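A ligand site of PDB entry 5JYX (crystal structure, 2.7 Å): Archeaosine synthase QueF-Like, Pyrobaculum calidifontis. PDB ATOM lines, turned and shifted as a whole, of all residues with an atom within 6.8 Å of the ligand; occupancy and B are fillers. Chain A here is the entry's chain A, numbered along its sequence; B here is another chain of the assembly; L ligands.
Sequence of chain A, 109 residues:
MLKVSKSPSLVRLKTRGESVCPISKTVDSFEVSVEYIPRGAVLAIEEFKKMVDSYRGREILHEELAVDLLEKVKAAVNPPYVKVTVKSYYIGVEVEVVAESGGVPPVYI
The backbone NH (N) of Ile 45 of chain B lies within hydrogen-bond range of a nitrogen (N4) of the ligand, 3.2 Å away.
A nitrogen (N2) of the ligand is in hydrogen-bond range of the side-chain carboxylate of Glu 63 (2.7 Å).
The side-chain carboxylate of Glu 46 of chain B sits at hydrogen-bond distance from a nitrogen (N5) of the ligand, at 2.9 Å.
N1 of the ligand lies within hydrogen-bond range of OD2 of Asp 28 (2.6 Å).
The backbone carbonyl oxygen of Leu 43 of chain B lies within hydrogen-bond range of a nitrogen (N3) of the ligand (2.9 Å).
The backbone NH (N) of His 62 lies within hydrogen-bond range of an oxygen (O1) of the ligand (3.0 Å).
ND1 of His 62 is in hydrogen-bond range of O1 of the ligand, at 3.4 Å.
C4 of the ligand is covalently linked to SG of Cys 21.
The backbone NH of Asp 28 lies within hydrogen-bond range of the backbone carbonyl oxygen of Ser 19 (2.9 Å).
OG of Ser 24 is in hydrogen-bond range of OH of Tyr 90, 2.7 Å away.
OG of Ser 88 lies within hydrogen-bond range of NE2 of His 62 (3.0 Å).
The backbone carbonyl oxygen of Thr 26 is in hydrogen-bond range of the backbone NH of Cys 21 (2.9 Å).
The backbone NH (N) of Leu 61 is in hydrogen-bond range of the side-chain carboxylate (OE1) of Glu 64, 3.0 Å away.
O of Val 42 of chain B lies within hydrogen-bond range of N of Leu 2 of chain B (3.2 Å).
OH of Tyr 36 of chain B is in hydrogen-bond range of N of Leu 43 of chain B (2.8 Å).
Merely in contact with the ligand: Ile 23, Leu 61, Tyr 90, Leu 2 of chain B, Val 42 of chain B and Ala 44 of chain B.
Hydrophobic or aromatic side chains within 4 Å of the ligand: Ile 23, Leu 61, His 62, Tyr 90, Leu 2 of chain B, Val 42 of chain B and Ile 45 of chain B.
13 residues have an atom within 4 Å of the ligand: Cys 21, Ile 23, Asp 28, Leu 61, His 62, Glu 63, Tyr 90, Leu 2 of chain B, Val 42 of chain B, Leu 43 of chain B, Ala 44 of chain B, Ile 45 of chain B and Glu 46 of chain B.
The nearest printed residue that does not touch the ligand is Pro 22 (4.2 Å).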
ATOM      1  N   SER A  19      13.816 -25.404   9.960  1.00  0.00           N
ATOM      2  CA  SER A  19      14.521 -26.062  11.022  1.00  0.00           C
ATOM      3  C   SER A  19      13.657 -26.012  12.266  1.00  0.00           C
ATOM      4  O   SER A  19      12.486 -25.703  12.187  1.00  0.00           O
ATOM      5  CB  SER A  19      15.870 -25.374  11.236  1.00  0.00           C
ATOM      6  OG  SER A  19      15.723 -24.006  11.638  1.00  0.00           O
ATOM      7  N   VAL A  20      14.233 -26.357  13.409  1.00  0.00           N
ATOM      8  CA  VAL A  20      13.530 -26.232  14.667  1.00  0.00           C
ATOM      9  C   VAL A  20      14.304 -25.345  15.647  1.00  0.00           C
ATOM     10  O   VAL A  20      15.538 -25.426  15.763  1.00  0.00           O
ATOM     11  CB  VAL A  20      13.286 -27.633  15.265  1.00  0.00           C
ATOM     12  CG1 VAL A  20      12.545 -27.505  16.598  1.00  0.00           C
ATOM     13  CG2 VAL A  20      12.513 -28.495  14.253  1.00  0.00           C
ATOM     14  N   CYS A  21      13.575 -24.493  16.349  1.00  0.00           N
ATOM     15  CA  CYS A  21      14.179 -23.581  17.291  1.00  0.00           C
ATOM     16  C   CYS A  21      14.370 -24.411  18.516  1.00  0.00           C
ATOM     17  O   CYS A  21      13.426 -24.985  18.995  1.00  0.00           O
ATOM     18  CB  CYS A  21      13.222 -22.427  17.585  1.00  0.00           C
ATOM     19  SG  CYS A  21      14.050 -20.998  18.325  1.00  0.00           S
ATOM     20  N   PRO A  22      15.597 -24.513  19.016  1.00  0.00           N
ATOM     21  CA  PRO A  22      15.778 -25.352  20.221  1.00  0.00           C
ATOM     22  C   PRO A  22      15.038 -24.831  21.476  1.00  0.00           C
ATOM     23  O   PRO A  22      14.527 -25.629  22.281  1.00  0.00           O
ATOM     24  CB  PRO A  22      17.293 -25.318  20.448  1.00  0.00           C
ATOM     25  CG  PRO A  22      17.871 -24.413  19.451  1.00  0.00           C
ATOM     26  CD  PRO A  22      16.772 -23.669  18.751  1.00  0.00           C
ATOM     27  N   ILE A  23      15.005 -23.506  21.636  1.00  0.00           N
ATOM     28  CA  ILE A  23      14.321 -22.883  22.757  1.00  0.00           C
ATOM     29  C   ILE A  23      12.854 -23.404  22.778  1.00  0.00           C
ATOM     30  O   ILE A  23      12.539 -24.378  23.458  1.00  0.00           O
ATOM     31  CB  ILE A  23      14.475 -21.317  22.732  1.00  0.00           C
ATOM     32  CG1 ILE A  23      15.901 -20.853  23.206  1.00  0.00           C
ATOM     33  CG2 ILE A  23      13.392 -20.634  23.543  1.00  0.00           C
ATOM     34  CD1 ILE A  23      17.050 -20.908  22.158  1.00  0.00           C
ATOM     35  N   SER A  24      12.007 -22.832  21.933  1.00  0.00           N
ATOM     36  CA  SER A  24      10.590 -23.171  21.893  1.00  0.00           C
ATOM     37  C   SER A  24      10.167 -24.387  21.092  1.00  0.00           C
ATOM     38  O   SER A  24       9.023 -24.685  21.083  1.00  0.00           O
ATOM     39  CB  SER A  24       9.825 -21.955  21.364  1.00  0.00           C
ATOM     40  OG  SER A  24      10.065 -21.748  19.974  1.00  0.00           O
ATOM     41  N   THR A  26       9.528 -24.884  18.017  1.00  0.00           N
ATOM     42  CA  THR A  26       8.747 -24.562  16.860  1.00  0.00           C
ATOM     43  C   THR A  26       9.599 -24.592  15.593  1.00  0.00           C
ATOM     44  O   THR A  26      10.815 -24.497  15.615  1.00  0.00           O
ATOM     45  CB  THR A  26       8.115 -23.163  16.989  1.00  0.00           C
ATOM     46  OG1 THR A  26       9.006 -22.235  17.590  1.00  0.00           O
ATOM     47  CG2 THR A  26       6.949 -23.239  17.836  1.00  0.00           C
ATOM     48  N   ASP A  28      11.066 -23.126  12.171  1.00  0.00           N
ATOM     49  CA  ASP A  28      11.627 -21.805  11.789  1.00  0.00           C
ATOM     50  C   ASP A  28      11.836 -21.837  10.331  1.00  0.00           C
ATOM     51  O   ASP A  28      12.606 -22.627   9.890  1.00  0.00           O
ATOM     52  CB  ASP A  28      13.004 -21.619  12.440  1.00  0.00           C
ATOM     53  CG  ASP A  28      12.923 -20.950  13.833  1.00  0.00           C
ATOM     54  OD1 ASP A  28      11.911 -20.224  14.077  1.00  0.00           O
ATOM     55  OD2 ASP A  28      13.878 -21.153  14.662  1.00  0.00           O
ATOM     56  N   ILE A  60      18.361 -26.365  15.974  1.00  0.00           N
ATOM     57  CA  ILE A  60      19.648 -25.676  15.683  1.00  0.00           C
ATOM     58  C   ILE A  60      19.394 -24.178  15.577  1.00  0.00           C
ATOM     59  O   ILE A  60      18.357 -23.787  15.064  1.00  0.00           O
ATOM     60  CB  ILE A  60      20.269 -26.267  14.396  1.00  0.00           C
ATOM     61  CG1 ILE A  60      21.626 -25.693  14.097  1.00  0.00           C
ATOM     62  CG2 ILE A  60      19.343 -26.111  13.221  1.00  0.00           C
ATOM     63  CD1 ILE A  60      22.266 -26.336  12.884  1.00  0.00           C
ATOM     64  N   LEU A  61      20.313 -23.367  16.079  1.00  0.00           N
ATOM     65  CA  LEU A  61      20.173 -21.915  15.968  1.00  0.00           C
ATOM     66  C   LEU A  61      20.606 -21.560  14.573  1.00  0.00           C
ATOM     67  O   LEU A  61      21.370 -22.263  13.985  1.00  0.00           O
ATOM     68  CB  LEU A  61      21.069 -21.180  16.951  1.00  0.00           C
ATOM     69  CG  LEU A  61      21.031 -21.589  18.472  1.00  0.00           C
ATOM     70  CD1 LEU A  61      22.280 -21.052  19.132  1.00  0.00           C
ATOM     71  CD2 LEU A  61      19.794 -21.025  19.148  1.00  0.00           C
ATOM     72  N   HIS A  62      20.122 -20.437  14.060  1.00  0.00           N
ATOM     73  CA  HIS A  62      20.434 -19.996  12.713  1.00  0.00           C
ATOM     74  C   HIS A  62      21.899 -19.674  12.541  1.00  0.00           C
ATOM     75  O   HIS A  62      22.421 -19.745  11.468  1.00  0.00           O
ATOM     76  CB  HIS A  62      19.619 -18.736  12.315  1.00  0.00           C
ATOM     77  CG  HIS A  62      18.153 -18.963  12.270  1.00  0.00           C
ATOM     78  ND1 HIS A  62      17.253 -18.119  12.896  1.00  0.00           N
ATOM     79  CD2 HIS A  62      17.425 -19.987  11.752  1.00  0.00           C
ATOM     80  CE1 HIS A  62      16.031 -18.600  12.744  1.00  0.00           C
ATOM     81  NE2 HIS A  62      16.113 -19.727  12.032  1.00  0.00           N
ATOM     82  N   GLU A  63      22.543 -19.245  13.609  1.00  0.00           N
ATOM     83  CA  GLU A  63      23.957 -18.909  13.608  1.00  0.00           C
ATOM     84  C   GLU A  63      24.736 -20.199  13.405  1.00  0.00           C
ATOM     85  O   GLU A  63      25.741 -20.216  12.719  1.00  0.00           O
ATOM     86  CB  GLU A  63      24.315 -18.237  14.935  1.00  0.00           C
ATOM     87  CG  GLU A  63      23.702 -16.831  15.121  1.00  0.00           C
ATOM     88  CD  GLU A  63      22.260 -16.744  15.753  1.00  0.00           C
ATOM     89  OE1 GLU A  63      21.574 -17.826  15.796  1.00  0.00           O
ATOM     90  OE2 GLU A  63      21.830 -15.577  16.205  1.00  0.00           O
ATOM     91  N   GLU A  64      24.259 -21.276  14.025  1.00  0.00           N
ATOM     92  CA  GLU A  64      24.829 -22.613  13.903  1.00  0.00           C
ATOM     93  C   GLU A  64      24.657 -23.187  12.482  1.00  0.00           C
ATOM     94  O   GLU A  64      25.585 -23.810  11.924  1.00  0.00           O
ATOM     95  CB  GLU A  64      24.162 -23.547  14.912  1.00  0.00           C
ATOM     96  CG  GLU A  64      24.919 -23.702  16.232  1.00  0.00           C
ATOM     97  CD  GLU A  64      24.026 -23.997  17.452  1.00  0.00           C
ATOM     98  OE1 GLU A  64      22.831 -24.500  17.323  1.00  0.00           O
ATOM     99  OE2 GLU A  64      24.570 -23.683  18.554  1.00  0.00           O
ATOM    100  N   SER A  88      15.951 -15.032   8.489  1.00  0.00           N
ATOM    101  CA  SER A  88      14.889 -15.657   9.252  1.00  0.00           C
ATOM    102  C   SER A  88      14.150 -14.601  10.020  1.00  0.00           C
ATOM    103  O   SER A  88      14.404 -13.458   9.817  1.00  0.00           O
ATOM    104  CB  SER A  88      15.512 -16.678  10.161  1.00  0.00           C
ATOM    105  OG  SER A  88      14.762 -17.871  10.105  1.00  0.00           O
ATOM    106  N   TYR A  90      11.985 -14.359  13.889  1.00  0.00           N
ATOM    107  CA  TYR A  90      11.528 -14.974  15.124  1.00  0.00           C
ATOM    108  C   TYR A  90      11.019 -13.893  16.085  1.00  0.00           C
ATOM    109  O   TYR A  90      11.706 -12.921  16.410  1.00  0.00           O
ATOM    110  CB  TYR A  90      12.629 -15.834  15.775  1.00  0.00           C
ATOM    111  CG  TYR A  90      12.135 -16.720  16.915  1.00  0.00           C
ATOM    112  CD1 TYR A  90      11.106 -17.636  16.718  1.00  0.00           C
ATOM    113  CD2 TYR A  90      12.741 -16.647  18.175  1.00  0.00           C
ATOM    114  CE1 TYR A  90      10.658 -18.450  17.752  1.00  0.00           C
ATOM    115  CE2 TYR A  90      12.327 -17.438  19.241  1.00  0.00           C
ATOM    116  CZ  TYR A  90      11.272 -18.344  19.063  1.00  0.00           C
ATOM    117  OH  TYR A  90      10.834 -19.122  20.188  1.00  0.00           O
ATOM    118  N   ILE A  91       9.769 -14.066  16.491  1.00  0.00           N
ATOM    119  CA  ILE A  91       9.135 -13.271  17.480  1.00  0.00           C
ATOM    120  C   ILE A  91       9.360 -11.779  17.264  1.00  0.00           C
ATOM    121  O   ILE A  91       9.625 -10.989  18.225  1.00  0.00           O
ATOM    122  CB  ILE A  91       9.503 -13.798  18.891  1.00  0.00           C
ATOM    123  CG1 ILE A  91      10.982 -13.624  19.261  1.00  0.00           C
ATOM    124  CG2 ILE A  91       9.109 -15.274  18.999  1.00  0.00           C
ATOM    125  CD1 ILE A  91      11.280 -13.851  20.720  1.00  0.00           C
ATOM    126  N   VAL A  95      16.308 -11.556  11.236  1.00  0.00           N
ATOM    127  CA  VAL A  95      17.599 -12.141  11.551  1.00  0.00           C
ATOM    128  C   VAL A  95      18.370 -12.387  10.293  1.00  0.00           C
ATOM    129  O   VAL A  95      17.829 -12.976   9.385  1.00  0.00           O
ATOM    130  CB  VAL A  95      17.438 -13.526  12.189  1.00  0.00           C
ATOM    131  CG1 VAL A  95      18.785 -14.202  12.362  1.00  0.00           C
ATOM    132  CG2 VAL A  95      16.749 -13.394  13.541  1.00  0.00           C
ATOM    133  N   LEU B   2      24.011 -17.254  24.188  1.00  0.00           N
ATOM    134  CA  LEU B   2      24.192 -18.670  23.852  1.00  0.00           C
ATOM    135  C   LEU B   2      25.537 -18.916  23.170  1.00  0.00           C
ATOM    136  O   LEU B   2      25.895 -18.180  22.236  1.00  0.00           O
ATOM    137  CB  LEU B   2      23.058 -19.121  22.898  1.00  0.00           C
ATOM    138  CG  LEU B   2      21.607 -18.677  23.173  1.00  0.00           C
ATOM    139  CD1 LEU B   2      21.090 -17.810  22.038  1.00  0.00           C
ATOM    140  CD2 LEU B   2      20.691 -19.883  23.351  1.00  0.00           C
ATOM    141  N   VAL B  11      26.255 -11.013  12.191  1.00  0.00           N
ATOM    142  CA  VAL B  11      24.811 -11.162  12.532  1.00  0.00           C
ATOM    143  C   VAL B  11      24.143  -9.800  12.518  1.00  0.00           C
ATOM    144  O   VAL B  11      24.696  -8.869  13.071  1.00  0.00           O
ATOM    145  CB  VAL B  11      24.602 -11.771  13.945  1.00  0.00           C
ATOM    146  CG1 VAL B  11      23.137 -11.797  14.365  1.00  0.00           C
ATOM    147  CG2 VAL B  11      25.136 -13.179  13.981  1.00  0.00           C
ATOM    148  N   LEU B  13      20.356  -8.196  13.549  1.00  0.00           N
ATOM    149  CA  LEU B  13      19.045  -8.359  14.098  1.00  0.00           C
ATOM    150  C   LEU B  13      18.269  -7.069  13.900  1.00  0.00           C
ATOM    151  O   LEU B  13      18.815  -6.030  13.995  1.00  0.00           O
ATOM    152  CB  LEU B  13      19.150  -8.634  15.551  1.00  0.00           C
ATOM    153  CG  LEU B  13      20.005  -9.807  15.941  1.00  0.00           C
ATOM    154  CD1 LEU B  13      20.141  -9.785  17.444  1.00  0.00           C
ATOM    155  CD2 LEU B  13      19.414 -11.109  15.495  1.00  0.00           C
ATOM    156  N   TYR B  36      26.680  -7.049  14.130  1.00  0.00           N
ATOM    157  CA  TYR B  36      27.800  -7.290  15.050  1.00  0.00           C
ATOM    158  C   TYR B  36      28.619  -8.496  14.635  1.00  0.00           C
ATOM    159  O   TYR B  36      28.083  -9.440  14.036  1.00  0.00           O
ATOM    160  CB  TYR B  36      27.315  -7.388  16.511  1.00  0.00           C
ATOM    161  CG  TYR B  36      26.626  -8.709  16.925  1.00  0.00           C
ATOM    162  CD1 TYR B  36      25.248  -8.922  16.756  1.00  0.00           C
ATOM    163  CD2 TYR B  36      27.355  -9.747  17.500  1.00  0.00           C
ATOM    164  CE1 TYR B  36      24.634 -10.094  17.123  1.00  0.00           C
ATOM    165  CE2 TYR B  36      26.741 -10.925  17.875  1.00  0.00           C
ATOM    166  CZ  TYR B  36      25.380 -11.105  17.682  1.00  0.00           C
ATOM    167  OH  TYR B  36      24.821 -12.303  18.069  1.00  0.00           O
ATOM    168  N   VAL B  42      26.904 -15.387  21.030  1.00  0.00           N
ATOM    169  CA  VAL B  42      25.894 -14.855  20.185  1.00  0.00           C
ATOM    170  C   VAL B  42      24.698 -14.377  21.011  1.00  0.00           C
ATOM    171  O   VAL B  42      24.192 -15.074  21.893  1.00  0.00           O
ATOM    172  CB  VAL B  42      25.477 -15.969  19.249  1.00  0.00           C
ATOM    173  CG1 VAL B  42      24.030 -15.824  18.796  1.00  0.00           C
ATOM    174  CG2 VAL B  42      26.455 -16.060  18.079  1.00  0.00           C
ATOM    175  N   LEU B  43      24.222 -13.191  20.697  1.00  0.00           N
ATOM    176  CA  LEU B  43      23.133 -12.575  21.444  1.00  0.00           C
ATOM    177  C   LEU B  43      21.830 -13.321  21.176  1.00  0.00           C
ATOM    178  O   LEU B  43      21.450 -13.511  20.025  1.00  0.00           O
ATOM    179  CB  LEU B  43      22.998 -11.102  21.035  1.00  0.00           C
ATOM    180  CG  LEU B  43      21.974 -10.239  21.796  1.00  0.00           C
ATOM    181  CD1 LEU B  43      22.293 -10.184  23.294  1.00  0.00           C
ATOM    182  CD2 LEU B  43      21.894  -8.821  21.234  1.00  0.00           C
ATOM    183  N   ALA B  44      21.159 -13.742  22.235  1.00  0.00           N
ATOM    184  CA  ALA B  44      19.860 -14.397  22.036  1.00  0.00           C
ATOM    185  C   ALA B  44      18.842 -13.380  21.571  1.00  0.00           C
ATOM    186  O   ALA B  44      18.852 -12.221  21.972  1.00  0.00           O
ATOM    187  CB  ALA B  44      19.379 -15.131  23.279  1.00  0.00           C
ATOM    188  N   ILE B  45      17.971 -13.829  20.692  1.00  0.00           N
ATOM    189  CA  ILE B  45      17.000 -12.956  20.145  1.00  0.00           C
ATOM    190  C   ILE B  45      16.081 -12.509  21.235  1.00  0.00           C
ATOM    191  O   ILE B  45      15.655 -11.369  21.240  1.00  0.00           O
ATOM    192  CB  ILE B  45      16.195 -13.654  19.055  1.00  0.00           C
ATOM    193  CG1 ILE B  45      17.097 -13.915  17.854  1.00  0.00           C
ATOM    194  CG2 ILE B  45      14.975 -12.826  18.640  1.00  0.00           C
ATOM    195  CD1 ILE B  45      16.428 -14.844  16.834  1.00  0.00           C
ATOM    196  N   GLU B  46      15.727 -13.403  22.138  1.00  0.00           N
ATOM    197  CA  GLU B  46      14.882 -13.020  23.283  1.00  0.00           C
ATOM    198  C   GLU B  46      15.505 -11.850  24.082  1.00  0.00           C
ATOM    199  O   GLU B  46      14.780 -10.943  24.500  1.00  0.00           O
ATOM    200  CB  GLU B  46      14.646 -14.211  24.216  1.00  0.00           C
ATOM    201  CG  GLU B  46      13.727 -15.300  23.654  1.00  0.00           C
ATOM    202  CD  GLU B  46      14.437 -16.385  22.825  1.00  0.00           C
ATOM    203  OE1 GLU B  46      15.649 -16.249  22.465  1.00  0.00           O
ATOM    204  OE2 GLU B  46      13.717 -17.418  22.565  1.00  0.00           O
HETATM  205  O1  LIG L   1      18.343 -19.064  15.991  1.00  0.00           O
HETATM  206  C1  LIG L   1      18.360 -18.285  17.122  1.00  0.00           C
HETATM  207  C2  LIG L   1      17.245 -18.332  18.118  1.00  0.00           C
HETATM  208  C3  LIG L   1      16.014 -18.964  18.379  1.00  0.00           C
HETATM  209  C4  LIG L   1      15.194 -19.954  17.594  1.00  0.00           C
HETATM  210  N1  LIG L   1      15.531 -20.170  16.404  1.00  0.00           N
HETATM  211  N2  LIG L   1      19.418 -17.445  17.375  1.00  0.00           N
HETATM  212  C5  LIG L   1      19.453 -16.686  18.491  1.00  0.00           C
HETATM  213  N3  LIG L   1      20.498 -15.854  18.675  1.00  0.00           N
HETATM  214  N4  LIG L   1      18.454 -16.695  19.434  1.00  0.00           N
HETATM  215  C6  LIG L   1      17.399 -17.489  19.227  1.00  0.00           C
HETATM  216  N5  LIG L   1      16.349 -17.592  20.046  1.00  0.00           N
HETATM  217  C7  LIG L   1      15.457 -18.471  19.544  1.00  0.00           C
